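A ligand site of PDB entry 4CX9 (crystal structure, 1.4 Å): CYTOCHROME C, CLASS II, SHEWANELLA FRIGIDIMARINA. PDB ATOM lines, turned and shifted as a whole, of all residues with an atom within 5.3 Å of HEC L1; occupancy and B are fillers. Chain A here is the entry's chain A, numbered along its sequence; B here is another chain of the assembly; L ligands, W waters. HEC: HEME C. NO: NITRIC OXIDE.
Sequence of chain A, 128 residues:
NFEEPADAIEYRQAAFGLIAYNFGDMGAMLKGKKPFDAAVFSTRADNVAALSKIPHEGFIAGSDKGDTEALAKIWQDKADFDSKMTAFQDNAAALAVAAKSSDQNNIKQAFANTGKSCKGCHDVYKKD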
ATOM      1  N   ILE A   9     -11.999 -14.175  23.286  1.00  0.00           N
ATOM      2  CA  ILE A   9     -12.024 -15.330  24.142  1.00  0.00           C
ATOM      3  C   ILE A   9     -13.411 -15.967  24.279  1.00  0.00           C
ATOM      4  O   ILE A   9     -13.602 -17.185  24.114  1.00  0.00           O
ATOM      5  CB  ILE A   9     -11.455 -14.985  25.554  1.00  0.00           C
ATOM      6  CG1 ILE A   9      -9.978 -14.702  25.420  1.00  0.00           C
ATOM      7  CG2 ILE A   9     -11.654 -16.144  26.486  1.00  0.00           C
ATOM      8  CD1 ILE A   9      -9.385 -13.937  26.635  1.00  0.00           C
ATOM      9  N   ARG A  12     -14.433 -17.786  20.899  1.00  0.00           N
ATOM     10  CA  ARG A  12     -13.891 -19.117  20.647  1.00  0.00           C
ATOM     11  C   ARG A  12     -14.422 -20.131  21.662  1.00  0.00           C
ATOM     12  O   ARG A  12     -14.665 -21.283  21.335  1.00  0.00           O
ATOM     13  CB  ARG A  12     -12.330 -19.077  20.606  1.00  0.00           C
ATOM     14  CG  ARG A  12     -11.619 -18.879  21.953  1.00  0.00           C
ATOM     15  CD  ARG A  12     -10.333 -18.105  21.770  1.00  0.00           C
ATOM     16  NE  ARG A  12      -9.516 -18.088  22.990  1.00  0.00           N
ATOM     17  CZ  ARG A  12      -8.483 -17.246  23.149  1.00  0.00           C
ATOM     18  NH1 ARG A  12      -8.218 -16.325  22.242  1.00  0.00           N
ATOM     19  NH2 ARG A  12      -7.758 -17.304  24.244  1.00  0.00           N
ATOM     20  N   GLN A  13     -14.578 -19.709  22.926  1.00  0.00           N
ATOM     21  CA  GLN A  13     -15.136 -20.590  23.978  1.00  0.00           C
ATOM     22  C   GLN A  13     -16.557 -21.045  23.618  1.00  0.00           C
ATOM     23  O   GLN A  13     -16.894 -22.227  23.743  1.00  0.00           O
ATOM     24  CB  GLN A  13     -15.099 -19.922  25.350  1.00  0.00           C
ATOM     25  CG  GLN A  13     -13.685 -19.842  25.912  1.00  0.00           C
ATOM     26  CD  GLN A  13     -13.586 -19.134  27.240  1.00  0.00           C
ATOM     27  OE1 GLN A  13     -14.451 -18.340  27.600  1.00  0.00           O
ATOM     28  NE2 GLN A  13     -12.467 -19.366  27.937  1.00  0.00           N
ATOM     29  N   PHE A  16     -16.387 -23.628  20.799  1.00  0.00           N
ATOM     30  CA  PHE A  16     -16.005 -24.949  21.274  1.00  0.00           C
ATOM     31  C   PHE A  16     -17.091 -25.647  22.106  1.00  0.00           C
ATOM     32  O   PHE A  16     -17.232 -26.864  22.053  1.00  0.00           O
ATOM     33  CB  PHE A  16     -14.650 -24.878  22.067  1.00  0.00           C
ATOM     34  CG  PHE A  16     -13.434 -24.763  21.177  1.00  0.00           C
ATOM     35  CD1 PHE A  16     -13.155 -25.731  20.229  1.00  0.00           C
ATOM     36  CD2 PHE A  16     -12.554 -23.693  21.337  1.00  0.00           C
ATOM     37  CE1 PHE A  16     -12.011 -25.612  19.407  1.00  0.00           C
ATOM     38  CE2 PHE A  16     -11.452 -23.575  20.517  1.00  0.00           C
ATOM     39  CZ  PHE A  16     -11.206 -24.542  19.569  1.00  0.00           C
ATOM     40  N   GLY A  17     -17.834 -24.913  22.917  1.00  0.00           N
ATOM     41  CA  GLY A  17     -18.909 -25.500  23.640  1.00  0.00           C
ATOM     42  C   GLY A  17     -19.945 -26.118  22.726  1.00  0.00           C
ATOM     43  O   GLY A  17     -20.436 -27.215  23.004  1.00  0.00           O
ATOM     44  N   ILE A  19     -19.391 -27.137  19.623  1.00  0.00           N
ATOM     45  CA  ILE A  19     -18.728 -28.303  19.034  1.00  0.00           C
ATOM     46  C   ILE A  19     -18.857 -29.461  19.987  1.00  0.00           C
ATOM     47  O   ILE A  19     -19.190 -30.593  19.585  1.00  0.00           O
ATOM     48  CB  ILE A  19     -17.253 -27.973  18.740  1.00  0.00           C
ATOM     49  CG1 ILE A  19     -17.171 -27.038  17.552  1.00  0.00           C
ATOM     50  CG2 ILE A  19     -16.465 -29.229  18.489  1.00  0.00           C
ATOM     51  CD1 ILE A  19     -15.808 -26.409  17.346  1.00  0.00           C
ATOM     52  N   ALA A  20     -18.548 -29.251  21.261  1.00  0.00           N
ATOM     53  CA  ALA A  20     -18.521 -30.357  22.217  1.00  0.00           C
ATOM     54  C   ALA A  20     -19.904 -30.983  22.430  1.00  0.00           C
ATOM     55  O   ALA A  20     -20.035 -32.199  22.600  1.00  0.00           O
ATOM     56  CB  ALA A  20     -17.941 -29.902  23.521  1.00  0.00           C
ATOM     57  N   PHE A  23     -20.557 -33.011  19.070  1.00  0.00           N
ATOM     58  CA  PHE A  23     -19.619 -34.163  19.040  1.00  0.00           C
ATOM     59  C   PHE A  23     -19.963 -35.177  20.113  1.00  0.00           C
ATOM     60  O   PHE A  23     -19.886 -36.394  19.895  1.00  0.00           O
ATOM     61  CB  PHE A  23     -18.188 -33.640  19.143  1.00  0.00           C
ATOM     62  CG  PHE A  23     -17.154 -34.653  18.769  1.00  0.00           C
ATOM     63  CD1 PHE A  23     -16.987 -35.023  17.448  1.00  0.00           C
ATOM     64  CD2 PHE A  23     -16.331 -35.194  19.730  1.00  0.00           C
ATOM     65  CE1 PHE A  23     -16.055 -35.958  17.080  1.00  0.00           C
ATOM     66  CE2 PHE A  23     -15.375 -36.126  19.376  1.00  0.00           C
ATOM     67  CZ  PHE A  23     -15.241 -36.501  18.044  1.00  0.00           C
ATOM     68  N   VAL A  48     -20.798 -30.078  13.407  1.00  0.00           N
ATOM     69  CA  VAL A  48     -19.389 -30.052  13.787  1.00  0.00           C
ATOM     70  C   VAL A  48     -18.483 -29.568  12.679  1.00  0.00           C
ATOM     71  O   VAL A  48     -17.561 -28.789  12.914  1.00  0.00           O
ATOM     72  CB  VAL A  48     -18.911 -31.406  14.386  1.00  0.00           C
ATOM     73  CG1 VAL A  48     -17.435 -31.375  14.735  1.00  0.00           C
ATOM     74  CG2 VAL A  48     -19.689 -31.685  15.679  1.00  0.00           C
ATOM     75  N   PHE A  59      -8.453 -16.525  18.215  1.00  0.00           N
ATOM     76  CA  PHE A  59      -7.102 -16.651  18.763  1.00  0.00           C
ATOM     77  C   PHE A  59      -6.153 -15.502  18.393  1.00  0.00           C
ATOM     78  O   PHE A  59      -5.120 -15.667  17.738  1.00  0.00           O
ATOM     79  CB  PHE A  59      -6.536 -18.017  18.432  1.00  0.00           C
ATOM     80  CG  PHE A  59      -7.232 -19.134  19.210  1.00  0.00           C
ATOM     81  CD1 PHE A  59      -6.790 -19.502  20.447  1.00  0.00           C
ATOM     82  CD2 PHE A  59      -8.335 -19.819  18.678  1.00  0.00           C
ATOM     83  CE1 PHE A  59      -7.386 -20.488  21.200  1.00  0.00           C
ATOM     84  CE2 PHE A  59      -8.933 -20.835  19.425  1.00  0.00           C
ATOM     85  CZ  PHE A  59      -8.459 -21.182  20.689  1.00  0.00           C
ATOM     86  N   ASP A  67      -9.654 -14.484  31.061  1.00  0.00           N
ATOM     87  CA  ASP A  67     -10.288 -15.688  31.533  1.00  0.00           C
ATOM     88  C   ASP A  67     -10.302 -16.740  30.426  1.00  0.00           C
ATOM     89  O   ASP A  67     -11.345 -16.930  29.766  1.00  0.00           O
ATOM     90  CB  ASP A  67     -11.697 -15.359  31.990  1.00  0.00           C
ATOM     91  CG  ASP A  67     -12.412 -16.548  32.598  1.00  0.00           C
ATOM     92  OD1 ASP A  67     -11.771 -17.560  32.917  1.00  0.00           O
ATOM     93  OD2 ASP A  67     -13.669 -16.481  32.693  1.00  0.00           O
ATOM     94  N   THR A  68      -9.179 -17.409  30.278  1.00  0.00           N
ATOM     95  CA  THR A  68      -8.933 -18.361  29.173  1.00  0.00           C
ATOM     96  C   THR A  68      -8.111 -19.540  29.602  1.00  0.00           C
ATOM     97  O   THR A  68      -7.278 -19.465  30.530  1.00  0.00           O
ATOM     98  CB  THR A  68      -8.310 -17.630  27.961  1.00  0.00           C
ATOM     99  OG1 THR A  68      -8.199 -18.558  26.872  1.00  0.00           O
ATOM    100  CG2 THR A  68      -6.878 -17.123  28.264  1.00  0.00           C
ATOM    101  N   GLU A  69      -8.355 -20.671  28.948  1.00  0.00           N
ATOM    102  CA  GLU A  69      -7.533 -21.847  29.078  1.00  0.00           C
ATOM    103  C   GLU A  69      -6.576 -22.063  27.912  1.00  0.00           C
ATOM    104  O   GLU A  69      -5.935 -23.116  27.826  1.00  0.00           O
ATOM    105  CB  GLU A  69      -8.424 -23.107  29.224  1.00  0.00           C
ATOM    106  CG  GLU A  69      -9.542 -22.999  30.247  1.00  0.00           C
ATOM    107  CD  GLU A  69      -8.988 -22.814  31.641  1.00  0.00           C
ATOM    108  OE1 GLU A  69      -8.107 -23.629  32.021  1.00  0.00           O
ATOM    109  OE2 GLU A  69      -9.401 -21.818  32.305  1.00  0.00           O
ATOM    110  N   ALA A  70      -6.498 -21.082  27.034  1.00  0.00           N
ATOM    111  CA  ALA A  70      -5.551 -21.110  25.912  1.00  0.00           C
ATOM    112  C   ALA A  70      -4.171 -20.810  26.466  1.00  0.00           C
ATOM    113  O   ALA A  70      -3.997 -19.803  27.148  1.00  0.00           O
ATOM    114  CB  ALA A  70      -5.941 -20.100  24.847  1.00  0.00           C
ATOM    115  N   ILE A  74       0.388 -21.301  21.990  1.00  0.00           N
ATOM    116  CA  ILE A  74      -0.338 -21.035  20.736  1.00  0.00           C
ATOM    117  C   ILE A  74       0.351 -20.039  19.849  1.00  0.00           C
ATOM    118  O   ILE A  74       0.489 -20.253  18.667  1.00  0.00           O
ATOM    119  CB  ILE A  74      -1.791 -20.644  21.016  1.00  0.00           C
ATOM    120  CG1 ILE A  74      -2.511 -21.833  21.690  1.00  0.00           C
ATOM    121  CG2 ILE A  74      -2.502 -20.207  19.708  1.00  0.00           C
ATOM    122  CD1 ILE A  74      -3.900 -21.481  22.124  1.00  0.00           C
ATOM    123  N   PHE A  81      -0.282 -24.726  15.458  1.00  0.00           N
ATOM    124  CA  PHE A  81      -1.676 -24.549  15.856  1.00  0.00           C
ATOM    125  C   PHE A  81      -2.592 -24.495  14.639  1.00  0.00           C
ATOM    126  O   PHE A  81      -3.647 -25.164  14.674  1.00  0.00           O
ATOM    127  CB  PHE A  81      -1.826 -23.268  16.700  1.00  0.00           C
ATOM    128  CG  PHE A  81      -3.202 -23.050  17.272  1.00  0.00           C
ATOM    129  CD1 PHE A  81      -3.602 -23.730  18.402  1.00  0.00           C
ATOM    130  CD2 PHE A  81      -4.103 -22.176  16.675  1.00  0.00           C
ATOM    131  CE1 PHE A  81      -4.859 -23.505  18.980  1.00  0.00           C
ATOM    132  CE2 PHE A  81      -5.345 -21.957  17.215  1.00  0.00           C
ATOM    133  CZ  PHE A  81      -5.707 -22.595  18.384  1.00  0.00           C
ATOM    134  N   LYS A  84      -2.929 -27.870  12.938  1.00  0.00           N
ATOM    135  CA  LYS A  84      -3.839 -28.702  13.727  1.00  0.00           C
ATOM    136  C   LYS A  84      -5.293 -28.266  13.492  1.00  0.00           C
ATOM    137  O   LYS A  84      -6.193 -29.101  13.357  1.00  0.00           O
ATOM    138  CB  LYS A  84      -3.507 -28.651  15.228  1.00  0.00           C
ATOM    139  CG  LYS A  84      -2.295 -29.492  15.594  1.00  0.00           C
ATOM    140  CD  LYS A  84      -2.182 -29.490  17.101  1.00  0.00           C
ATOM    141  CE  LYS A  84      -0.908 -30.117  17.706  1.00  0.00           C
ATOM    142  NZ  LYS A  84      -0.386 -31.308  17.040  1.00  0.00           N
ATOM    143  N   MET A  85      -5.524 -26.951  13.535  1.00  0.00           N
ATOM    144  CA  MET A  85      -6.877 -26.442  13.326  1.00  0.00           C
ATOM    145  C   MET A  85      -7.423 -26.808  11.933  1.00  0.00           C
ATOM    146  O   MET A  85      -8.589 -27.226  11.822  1.00  0.00           O
ATOM    147  CB  MET A  85      -6.924 -24.941  13.488  1.00  0.00           C
ATOM    148  CG  MET A  85      -8.340 -24.399  13.509  1.00  0.00           C
ATOM    149  SD  MET A  85      -9.344 -24.859  14.954  1.00  0.00           S
ATOM    150  CE  MET A  85      -8.625 -23.793  16.214  1.00  0.00           C
ATOM    151  N   PHE A  88      -8.171 -30.429  11.780  1.00  0.00           N
ATOM    152  CA  PHE A  88      -9.459 -30.659  12.485  1.00  0.00           C
ATOM    153  C   PHE A  88     -10.642 -30.408  11.557  1.00  0.00           C
ATOM    154  O   PHE A  88     -11.544 -31.235  11.466  1.00  0.00           O
ATOM    155  CB  PHE A  88      -9.531 -29.759  13.738  1.00  0.00           C
ATOM    156  CG  PHE A  88     -10.891 -29.665  14.375  1.00  0.00           C
ATOM    157  CD1 PHE A  88     -11.679 -30.768  14.629  1.00  0.00           C
ATOM    158  CD2 PHE A  88     -11.340 -28.433  14.866  1.00  0.00           C
ATOM    159  CE1 PHE A  88     -12.898 -30.669  15.232  1.00  0.00           C
ATOM    160  CE2 PHE A  88     -12.549 -28.333  15.510  1.00  0.00           C
ATOM    161  CZ  PHE A  88     -13.328 -29.432  15.718  1.00  0.00           C
ATOM    162  N   THR A 114     -11.457 -37.659  14.210  1.00  0.00           N
ATOM    163  CA  THR A 114     -11.823 -36.270  14.643  1.00  0.00           C
ATOM    164  C   THR A 114     -11.513 -36.093  16.135  1.00  0.00           C
ATOM    165  O   THR A 114     -10.922 -35.085  16.534  1.00  0.00           O
ATOM    166  CB  THR A 114     -13.288 -35.970  14.350  1.00  0.00           C
ATOM    167  OG1 THR A 114     -13.531 -36.220  12.983  1.00  0.00           O
ATOM    168  CG2 THR A 114     -13.652 -34.554  14.692  1.00  0.00           C
ATOM    169  N   SER A 117      -7.931 -35.249  16.689  1.00  0.00           N
ATOM    170  CA  SER A 117      -7.722 -33.809  16.488  1.00  0.00           C
ATOM    171  C   SER A 117      -7.969 -33.025  17.794  1.00  0.00           C
ATOM    172  O   SER A 117      -7.170 -32.201  18.164  1.00  0.00           O
ATOM    173  CB  SER A 117      -8.575 -33.238  15.361  1.00  0.00           C
ATOM    174  OG  SER A 117      -7.996 -33.504  14.092  1.00  0.00           O
ATOM    175  N   CYS A 118      -9.092 -33.286  18.462  1.00  0.00           N
ATOM    176  CA  CYS A 118      -9.377 -32.625  19.711  1.00  0.00           C
ATOM    177  C   CYS A 118      -8.258 -32.860  20.707  1.00  0.00           C
ATOM    178  O   CYS A 118      -7.791 -31.890  21.341  1.00  0.00           O
ATOM    179  CB  CYS A 118     -10.676 -33.104  20.378  1.00  0.00           C
ATOM    180  SG  CYS A 118     -12.119 -33.425  19.369  1.00  0.00           S
ATOM    181  N   CYS A 121      -4.663 -31.271  19.926  1.00  0.00           N
ATOM    182  CA  CYS A 121      -4.550 -29.904  20.245  1.00  0.00           C
ATOM    183  C   CYS A 121      -4.684 -29.550  21.723  1.00  0.00           C
ATOM    184  O   CYS A 121      -3.884 -28.766  22.265  1.00  0.00           O
ATOM    185  CB  CYS A 121      -5.520 -29.134  19.358  1.00  0.00           C
ATOM    186  SG  CYS A 121      -5.298 -27.369  19.522  1.00  0.00           S
ATOM    187  N   HIS A 122      -5.672 -30.142  22.395  1.00  0.00           N
ATOM    188  CA  HIS A 122      -5.821 -30.036  23.825  1.00  0.00           C
ATOM    189  C   HIS A 122      -4.501 -30.250  24.568  1.00  0.00           C
ATOM    190  O   HIS A 122      -4.123 -29.458  25.429  1.00  0.00           O
ATOM    191  CB  HIS A 122      -6.860 -31.074  24.248  1.00  0.00           C
ATOM    192  CG  HIS A 122      -6.998 -31.218  25.729  1.00  0.00           C
ATOM    193  ND1 HIS A 122      -6.228 -32.090  26.455  1.00  0.00           N
ATOM    194  CD2 HIS A 122      -7.829 -30.615  26.616  1.00  0.00           C
ATOM    195  CE1 HIS A 122      -6.558 -32.009  27.734  1.00  0.00           C
ATOM    196  NE2 HIS A 122      -7.524 -31.119  27.857  1.00  0.00           N
ATOM    197  N   TYR A 125      -1.973 -27.271  23.621  1.00  0.00           N
ATOM    198  CA  TYR A 125      -2.313 -25.845  23.593  1.00  0.00           C
ATOM    199  C   TYR A 125      -3.368 -25.369  24.631  1.00  0.00           C
ATOM    200  O   TYR A 125      -3.668 -24.162  24.683  1.00  0.00           O
ATOM    201  CB  TYR A 125      -2.754 -25.479  22.183  1.00  0.00           C
ATOM    202  CG  TYR A 125      -1.640 -25.564  21.220  1.00  0.00           C
ATOM    203  CD1 TYR A 125      -0.544 -24.715  21.339  1.00  0.00           C
ATOM    204  CD2 TYR A 125      -1.635 -26.493  20.186  1.00  0.00           C
ATOM    205  CE1 TYR A 125       0.527 -24.835  20.457  1.00  0.00           C
ATOM    206  CE2 TYR A 125      -0.575 -26.581  19.260  1.00  0.00           C
ATOM    207  CZ  TYR A 125       0.498 -25.720  19.389  1.00  0.00           C
ATOM    208  OH  TYR A 125       1.578 -25.823  18.529  1.00  0.00           O
ATOM    209  N   LYS A 126      -3.926 -26.287  25.407  1.00  0.00           N
ATOM    210  CA  LYS A 126      -4.951 -25.972  26.434  1.00  0.00           C
ATOM    211  C   LYS A 126      -4.462 -26.346  27.805  1.00  0.00           C
ATOM    212  O   LYS A 126      -3.884 -27.408  27.984  1.00  0.00           O
ATOM    213  CB  LYS A 126      -6.281 -26.704  26.147  1.00  0.00           C
ATOM    214  CG  LYS A 126      -7.458 -26.218  26.969  1.00  0.00           C
ATOM    215  CD  LYS A 126      -8.745 -26.929  26.577  1.00  0.00           C
ATOM    216  CE  LYS A 126      -9.942 -26.412  27.316  1.00  0.00           C
ATOM    217  NZ  LYS A 126     -10.052 -26.961  28.702  1.00  0.00           N
ATOM    218  N   GLU B  10     -27.311 -21.697  28.055  1.00  0.00           N
ATOM    219  CA  GLU B  10     -25.955 -21.368  27.584  1.00  0.00           C
ATOM    220  C   GLU B  10     -25.796 -21.760  26.111  1.00  0.00           C
ATOM    221  O   GLU B  10     -25.178 -21.012  25.344  1.00  0.00           O
ATOM    222  CB  GLU B  10     -24.916 -22.133  28.407  1.00  0.00           C
ATOM    223  CG  GLU B  10     -23.468 -21.936  27.954  1.00  0.00           C
ATOM    224  CD  GLU B  10     -22.492 -22.700  28.829  1.00  0.00           C
ATOM    225  OE1 GLU B  10     -22.884 -23.071  29.979  1.00  0.00           O
ATOM    226  OE2 GLU B  10     -21.334 -22.925  28.378  1.00  0.00           O
HETATM  227 FE   HEC L   1     -10.971 -27.597  22.016  1.00  0.00          FE
HETATM  228  CHA HEC L   1     -11.499 -25.274  24.520  1.00  0.00           C
HETATM  229  CHB HEC L   1     -13.815 -29.173  22.956  1.00  0.00           C
HETATM  230  CHC HEC L   1     -10.894 -29.406  19.187  1.00  0.00           C
HETATM  231  CHD HEC L   1      -8.201 -26.008  21.146  1.00  0.00           C
HETATM  232  NA  HEC L   1     -12.385 -27.288  23.477  1.00  0.00           N
HETATM  233  C1A HEC L   1     -12.464 -26.299  24.387  1.00  0.00           C
HETATM  234  C2A HEC L   1     -13.578 -26.474  25.209  1.00  0.00           C
HETATM  235  C3A HEC L   1     -14.228 -27.603  24.803  1.00  0.00           C
HETATM  236  C4A HEC L   1     -13.477 -28.040  23.688  1.00  0.00           C
HETATM  237  CMA HEC L   1     -15.461 -28.244  25.382  1.00  0.00           C
HETATM  238  CAA HEC L   1     -13.958 -25.557  26.382  1.00  0.00           C
HETATM  239  CBA HEC L   1     -14.817 -24.386  25.877  1.00  0.00           C
HETATM  240  CGA HEC L   1     -15.303 -23.474  27.008  1.00  0.00           C
HETATM  241  O1A HEC L   1     -14.492 -22.701  27.491  1.00  0.00           O
HETATM  242  O2A HEC L   1     -16.522 -23.551  27.371  1.00  0.00           O
HETATM  243  NB  HEC L   1     -12.153 -29.002  21.229  1.00  0.00           N
HETATM  244  C1B HEC L   1     -13.208 -29.642  21.784  1.00  0.00           C
HETATM  245  C2B HEC L   1     -13.655 -30.756  21.037  1.00  0.00           C
HETATM  246  C3B HEC L   1     -12.865 -30.780  19.944  1.00  0.00           C
HETATM  247  C4B HEC L   1     -11.941 -29.726  20.086  1.00  0.00           C
HETATM  248  CMB HEC L   1     -14.774 -31.698  21.356  1.00  0.00           C
HETATM  249  CAB HEC L   1     -12.850 -31.734  18.783  1.00  0.00           C
HETATM  250  CBB HEC L   1     -14.177 -32.112  18.249  1.00  0.00           C
HETATM  251  NC  HEC L   1      -9.836 -27.635  20.371  1.00  0.00           N
HETATM  252  C1C HEC L   1      -9.877 -28.473  19.317  1.00  0.00           C
HETATM  253  C2C HEC L   1      -8.783 -28.268  18.411  1.00  0.00           C
HETATM  254  C3C HEC L   1      -8.004 -27.288  19.001  1.00  0.00           C
HETATM  255  C4C HEC L   1      -8.655 -26.950  20.213  1.00  0.00           C
HETATM  256  CMC HEC L   1      -8.596 -29.052  17.124  1.00  0.00           C
HETATM  257  CAC HEC L   1      -6.727 -26.690  18.495  1.00  0.00           C
HETATM  258  CBC HEC L   1      -6.456 -26.748  17.014  1.00  0.00           C
HETATM  259  ND  HEC L   1     -10.057 -25.890  22.707  1.00  0.00           N
HETATM  260  C1D HEC L   1      -8.854 -25.480  22.260  1.00  0.00           C
HETATM  261  C2D HEC L   1      -8.358 -24.411  23.056  1.00  0.00           C
HETATM  262  C3D HEC L   1      -9.348 -24.158  23.962  1.00  0.00           C
HETATM  263  C4D HEC L   1     -10.363 -25.096  23.745  1.00  0.00           C
HETATM  264  CMD HEC L   1      -7.030 -23.703  22.953  1.00  0.00           C
HETATM  265  CAD HEC L   1      -9.358 -23.099  25.026  1.00  0.00           C
HETATM  266  CBD HEC L   1     -10.170 -21.902  24.618  1.00  0.00           C
HETATM  267  CGD HEC L   1     -10.134 -20.777  25.649  1.00  0.00           C
HETATM  268  O1D HEC L   1     -10.296 -21.139  26.866  1.00  0.00           O
HETATM  269  O2D HEC L   1      -9.966 -19.606  25.265  1.00  0.00           O
HETATM  270  N    NO L   2     -10.006 -28.676  23.032  1.00  0.00           N
HETATM  271  O    NO L   2      -8.817 -28.667  23.200  1.00  0.00           O
HETATM  272  O   HOH W   1     -17.982 -25.725  27.291  1.00  0.00           O
HETATM  273  O   HOH W   2     -11.830 -23.187  27.672  1.00  0.00           O
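The side-chain sulfur of Cys 121 is bonded to a carbon (CAC) of HEC L1. O1D of HEC L1 lies within hydrogen-bond range of N of Glu 69, 2.9 Å away. SG of Cys 118 is covalently linked to CAB of HEC L1, at 1.9 Å. An oxygen (O2D) of HEC L1 sits at hydrogen-bond distance from the side-chain hydroxyl of Thr 68 (2.6 Å). The guanidinium group (NE) of Arg 12 lies within salt-bridge range of an oxygen (O2D) of HEC L1 (2.8 Å). An oxygen (O1D) of HEC L1 is in hydrogen-bond range of the side-chain amide nitrogen (NE2) of Gln 13 (3.0 Å).
N of NO L2 binds FE of HEC L1, 1.8 Å away.
The side-chain hydroxyl (OG1) of Thr 68 lies within hydrogen-bond range of the backbone NH (N) of Ala 70. The guanidinium group (NH2) of Arg 12 is in hydrogen-bond range of the side-chain hydroxyl (OG1) of Thr 68, 2.9 Å away. NE2 of Gln 13 lies within hydrogen-bond range of O of Asp 67 (3.2 Å).
Phe 16 touches HEC L1 (CE1 to NC, 3.1 Å). Ile 19 touches HEC L1 (CG2 to CBB, 3.7 Å). CB of Ala 20 touches CMA of HEC L1 (3.5 Å). CG of Phe 23 touches CBB of HEC L1, at 3.9 Å. Phe 59 touches HEC L1 (CZ to CMD, 3.7 Å). N of Ala 70 touches O1D of HEC L1, at 3.8 Å. Ile 74 touches HEC L1 (CD1 to CMD, 3.9 Å). Phe 81 touches HEC L1. Lys 84 touches HEC L1. Met 85 touches HEC L1. CE1 of Phe 88 touches CBB of HEC L1, 3.6 Å away. Ser 117 touches HEC L1. O of Tyr 125 touches CMD of HEC L1, 3.8 Å away. Lys 126 touches HEC L1 (CE to CHA, 3.4 Å). Hydrophobic or aromatic side chains that line HEC L1: Phe 16, Ile 19, Ala 20, Phe 23, Phe 59, Ile 74, Phe 81, Met 85 and Phe 88. Of the 27 residues printed, 20 come within 4 Å of HEC L1. Along chain A the residues within 4 Å of HEC L1 span positions 12 to 126.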
